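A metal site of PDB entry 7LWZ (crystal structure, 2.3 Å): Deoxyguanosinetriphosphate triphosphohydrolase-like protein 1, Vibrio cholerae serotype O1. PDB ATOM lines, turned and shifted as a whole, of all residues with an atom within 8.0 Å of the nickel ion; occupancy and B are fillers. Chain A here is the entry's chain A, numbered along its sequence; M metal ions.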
ATOM      1  N   ARG A  64     -15.314 -20.784 -23.628  1.00  0.00           N
ATOM      2  CA  ARG A  64     -16.580 -20.094 -23.844  1.00  0.00           C
ATOM      3  C   ARG A  64     -16.555 -19.321 -25.141  1.00  0.00           C
ATOM      4  O   ARG A  64     -17.618 -19.047 -25.719  1.00  0.00           O
ATOM      5  CB  ARG A  64     -16.846 -19.146 -22.683  1.00  0.00           C
ATOM      6  CG  ARG A  64     -17.053 -19.835 -21.365  1.00  0.00           C
ATOM      7  CD  ARG A  64     -18.515 -19.757 -20.999  1.00  0.00           C
ATOM      8  NE  ARG A  64     -18.661 -19.648 -19.556  1.00  0.00           N
ATOM      9  CZ  ARG A  64     -18.861 -20.676 -18.742  1.00  0.00           C
ATOM     10  NH1 ARG A  64     -18.938 -21.910 -19.252  1.00  0.00           N
ATOM     11  NH2 ARG A  64     -18.977 -20.476 -17.434  1.00  0.00           N
ATOM     12  N   HIS A  67     -17.299 -21.916 -27.818  1.00  0.00           N
ATOM     13  CA  HIS A  67     -18.725 -22.221 -27.691  1.00  0.00           C
ATOM     14  C   HIS A  67     -19.568 -21.140 -28.330  1.00  0.00           C
ATOM     15  O   HIS A  67     -20.588 -21.432 -28.969  1.00  0.00           O
ATOM     16  CB  HIS A  67     -19.129 -22.389 -26.221  1.00  0.00           C
ATOM     17  CG  HIS A  67     -20.602 -22.206 -25.950  1.00  0.00           C
ATOM     18  ND1 HIS A  67     -21.531 -23.189 -26.209  1.00  0.00           N
ATOM     19  CD2 HIS A  67     -21.292 -21.185 -25.396  1.00  0.00           C
ATOM     20  CE1 HIS A  67     -22.725 -22.778 -25.833  1.00  0.00           C
ATOM     21  NE2 HIS A  67     -22.613 -21.567 -25.324  1.00  0.00           N
ATOM     22  N   SER A  68     -19.158 -19.881 -28.182  1.00  0.00           N
ATOM     23  CA  SER A  68     -19.942 -18.787 -28.750  1.00  0.00           C
ATOM     24  C   SER A  68     -19.796 -18.706 -30.273  1.00  0.00           C
ATOM     25  O   SER A  68     -20.766 -18.408 -30.962  1.00  0.00           O
ATOM     26  CB  SER A  68     -19.518 -17.455 -28.097  1.00  0.00           C
ATOM     27  OG  SER A  68     -19.641 -17.505 -26.688  1.00  0.00           O
ATOM     28  N   ALA A  71     -22.149 -21.441 -31.563  1.00  0.00           N
ATOM     29  CA  ALA A  71     -23.541 -21.015 -31.487  1.00  0.00           C
ATOM     30  C   ALA A  71     -23.869 -20.033 -32.598  1.00  0.00           C
ATOM     31  O   ALA A  71     -24.915 -20.149 -33.265  1.00  0.00           O
ATOM     32  CB  ALA A  71     -23.850 -20.383 -30.128  1.00  0.00           C
ATOM     33  N   CYS A 103     -25.008 -14.342 -30.127  1.00  0.00           N
ATOM     34  CA  CYS A 103     -24.328 -15.547 -29.683  1.00  0.00           C
ATOM     35  C   CYS A 103     -22.912 -15.261 -29.242  1.00  0.00           C
ATOM     36  O   CYS A 103     -22.387 -15.953 -28.362  1.00  0.00           O
ATOM     37  CB  CYS A 103     -24.265 -16.598 -30.803  1.00  0.00           C
ATOM     38  SG  CYS A 103     -25.826 -17.046 -31.540  1.00  0.00           S
ATOM     39  N   HIS A 106     -23.621 -13.847 -25.504  1.00  0.00           N
ATOM     40  CA  HIS A 106     -24.549 -14.485 -24.557  1.00  0.00           C
ATOM     41  C   HIS A 106     -23.853 -14.930 -23.269  1.00  0.00           C
ATOM     42  O   HIS A 106     -24.481 -14.962 -22.212  1.00  0.00           O
ATOM     43  CB  HIS A 106     -25.303 -15.656 -25.230  1.00  0.00           C
ATOM     44  CG  HIS A 106     -24.636 -17.012 -25.139  1.00  0.00           C
ATOM     45  ND1 HIS A 106     -23.669 -17.434 -26.023  1.00  0.00           N
ATOM     46  CD2 HIS A 106     -24.849 -18.043 -24.284  1.00  0.00           C
ATOM     47  CE1 HIS A 106     -23.301 -18.672 -25.700  1.00  0.00           C
ATOM     48  NE2 HIS A 106     -23.996 -19.068 -24.652  1.00  0.00           N
ATOM     49  N   ASP A 107     -22.563 -15.235 -23.318  1.00  0.00           N
ATOM     50  CA  ASP A 107     -21.835 -15.754 -22.175  1.00  0.00           C
ATOM     51  C   ASP A 107     -20.891 -14.721 -21.556  1.00  0.00           C
ATOM     52  O   ASP A 107     -20.050 -15.084 -20.748  1.00  0.00           O
ATOM     53  CB  ASP A 107     -21.044 -16.992 -22.587  1.00  0.00           C
ATOM     54  CG  ASP A 107     -21.689 -18.276 -22.146  1.00  0.00           C
ATOM     55  OD1 ASP A 107     -22.199 -18.311 -21.021  1.00  0.00           O
ATOM     56  OD2 ASP A 107     -21.689 -19.248 -22.934  1.00  0.00           O
ATOM     57  N   HIS A 110     -20.588 -14.232 -17.462  1.00  0.00           N
ATOM     58  CA  HIS A 110     -20.305 -15.318 -16.551  1.00  0.00           C
ATOM     59  C   HIS A 110     -19.097 -14.978 -15.674  1.00  0.00           C
ATOM     60  O   HIS A 110     -18.135 -14.365 -16.145  1.00  0.00           O
ATOM     61  CB  HIS A 110     -20.103 -16.620 -17.320  1.00  0.00           C
ATOM     62  CG  HIS A 110     -21.391 -17.226 -17.788  1.00  0.00           C
ATOM     63  ND1 HIS A 110     -21.568 -18.576 -17.980  1.00  0.00           N
ATOM     64  CD2 HIS A 110     -22.589 -16.640 -18.077  1.00  0.00           C
ATOM     65  CE1 HIS A 110     -22.812 -18.805 -18.374  1.00  0.00           C
ATOM     66  NE2 HIS A 110     -23.446 -17.644 -18.447  1.00  0.00           N
ATOM     67  N   LYS A 165     -32.851 -12.452 -22.170  1.00  0.00           N
ATOM     68  CA  LYS A 165     -33.378 -13.802 -22.013  1.00  0.00           C
ATOM     69  C   LYS A 165     -34.417 -13.851 -20.906  1.00  0.00           C
ATOM     70  O   LYS A 165     -35.321 -14.696 -20.952  1.00  0.00           O
ATOM     71  CB  LYS A 165     -32.247 -14.769 -21.692  1.00  0.00           C
ATOM     72  CG  LYS A 165     -31.280 -15.009 -22.826  1.00  0.00           C
ATOM     73  CD  LYS A 165     -31.018 -16.496 -22.991  1.00  0.00           C
ATOM     74  CE  LYS A 165     -30.148 -17.078 -21.877  1.00  0.00           C
ATOM     75  NZ  LYS A 165     -29.900 -18.532 -22.102  1.00  0.00           N
ATOM     76  N   MET A 248     -31.336 -17.363 -30.777  1.00  0.00           N
ATOM     77  CA  MET A 248     -30.047 -17.516 -30.107  1.00  0.00           C
ATOM     78  C   MET A 248     -30.111 -18.626 -29.071  1.00  0.00           C
ATOM     79  O   MET A 248     -29.212 -19.459 -28.975  1.00  0.00           O
ATOM     80  CB  MET A 248     -29.642 -16.197 -29.475  1.00  0.00           C
ATOM     81  CG  MET A 248     -28.359 -16.239 -28.684  1.00  0.00           C
ATOM     82  SD  MET A 248     -28.722 -16.239 -26.925  1.00  0.00           S
ATOM     83  CE  MET A 248     -29.064 -14.507 -26.620  1.00  0.00           C
ATOM     84  N   GLU A 249     -31.223 -18.706 -28.336  1.00  0.00           N
ATOM     85  CA  GLU A 249     -31.363 -19.747 -27.318  1.00  0.00           C
ATOM     86  C   GLU A 249     -31.308 -21.144 -27.949  1.00  0.00           C
ATOM     87  O   GLU A 249     -30.681 -22.055 -27.392  1.00  0.00           O
ATOM     88  CB  GLU A 249     -32.669 -19.549 -26.533  1.00  0.00           C
ATOM     89  CG  GLU A 249     -32.615 -18.520 -25.407  1.00  0.00           C
ATOM     90  CD  GLU A 249     -33.761 -18.668 -24.414  1.00  0.00           C
ATOM     91  OE1 GLU A 249     -34.347 -19.771 -24.346  1.00  0.00           O
ATOM     92  OE2 GLU A 249     -34.067 -17.691 -23.693  1.00  0.00           O
ATOM     93  N   ALA A 251     -29.802 -21.929 -30.827  1.00  0.00           N
ATOM     94  CA  ALA A 251     -28.440 -22.180 -31.300  1.00  0.00           C
ATOM     95  C   ALA A 251     -27.511 -22.525 -30.136  1.00  0.00           C
ATOM     96  O   ALA A 251     -26.754 -23.505 -30.214  1.00  0.00           O
ATOM     97  CB  ALA A 251     -27.925 -20.966 -32.072  1.00  0.00           C
ATOM     98  N   ASP A 252     -27.607 -21.768 -29.038  1.00  0.00           N
ATOM     99  CA  ASP A 252     -26.839 -22.055 -27.834  1.00  0.00           C
ATOM    100  C   ASP A 252     -27.111 -23.479 -27.353  1.00  0.00           C
ATOM    101  O   ASP A 252     -26.181 -24.261 -27.137  1.00  0.00           O
ATOM    102  CB  ASP A 252     -27.208 -21.011 -26.777  1.00  0.00           C
ATOM    103  CG  ASP A 252     -26.333 -21.048 -25.526  1.00  0.00           C
ATOM    104  OD1 ASP A 252     -25.120 -21.324 -25.580  1.00  0.00           O
ATOM    105  OD2 ASP A 252     -26.894 -20.744 -24.453  1.00  0.00           O
ATOM    106  N   ASP A 253     -28.393 -23.867 -27.298  1.00  0.00           N
ATOM    107  CA  ASP A 253     -28.758 -25.200 -26.810  1.00  0.00           C
ATOM    108  C   ASP A 253     -28.233 -26.300 -27.731  1.00  0.00           C
ATOM    109  O   ASP A 253     -27.893 -27.393 -27.276  1.00  0.00           O
ATOM    110  CB  ASP A 253     -30.286 -25.326 -26.709  1.00  0.00           C
ATOM    111  CG  ASP A 253     -30.827 -24.961 -25.339  1.00  0.00           C
ATOM    112  OD1 ASP A 253     -30.063 -24.476 -24.467  1.00  0.00           O
ATOM    113  OD2 ASP A 253     -32.047 -25.158 -25.141  1.00  0.00           O
ATOM    114  N   ALA A 255     -25.489 -25.997 -29.726  1.00  0.00           N
ATOM    115  CA  ALA A 255     -24.034 -26.002 -29.532  1.00  0.00           C
ATOM    116  C   ALA A 255     -23.659 -26.743 -28.260  1.00  0.00           C
ATOM    117  O   ALA A 255     -22.804 -27.638 -28.274  1.00  0.00           O
ATOM    118  CB  ALA A 255     -23.520 -24.562 -29.420  1.00  0.00           C
ATOM    119  N   TYR A 256     -24.341 -26.436 -27.162  1.00  0.00           N
ATOM    120  CA  TYR A 256     -24.103 -27.145 -25.911  1.00  0.00           C
ATOM    121  C   TYR A 256     -24.336 -28.645 -26.089  1.00  0.00           C
ATOM    122  O   TYR A 256     -23.579 -29.461 -25.555  1.00  0.00           O
ATOM    123  CB  TYR A 256     -24.993 -26.539 -24.833  1.00  0.00           C
ATOM    124  CG  TYR A 256     -24.978 -27.207 -23.482  1.00  0.00           C
ATOM    125  CD1 TYR A 256     -23.977 -26.926 -22.541  1.00  0.00           C
ATOM    126  CD2 TYR A 256     -25.989 -28.081 -23.118  1.00  0.00           C
ATOM    127  CE1 TYR A 256     -23.987 -27.529 -21.267  1.00  0.00           C
ATOM    128  CE2 TYR A 256     -26.018 -28.683 -21.869  1.00  0.00           C
ATOM    129  CZ  TYR A 256     -25.020 -28.415 -20.945  1.00  0.00           C
ATOM    130  OH  TYR A 256     -25.078 -29.040 -19.699  1.00  0.00           O
HETATM  131 NI    NI M   1     -24.027 -20.969 -23.931  1.00  0.00          NI
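A ring nitrogen (ND1) of His 106 sits at hydrogen-bond distance from the backbone carbonyl oxygen (O) of Cys 103 (3.1 Å). The side-chain carboxylate of Asp 107 lies close to a ring nitrogen (NE2) of His 67, 3.5 Å away. NE2 of His 106 sits close to OD2 of Asp 107, at 2.9 Å. A ring nitrogen (NE2) of His 110 sits close to the side-chain carboxylate (OD1) of Asp 107, 2.9 Å away.
Asp 107 touches the nickel ion (OD2 to NI, 3.1 Å). Four residues have an atom within 4 Å of the nickel ion: His 67, His 106, Asp 107 and Asp 252.
The nickel ion is bound by OD1 of Asp 252 (2.0 Å), NE2 of His 106 (2.0 Å) and NE2 of His 67 (2.1 Å). The nickel ion has three donor atoms within binding distance.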
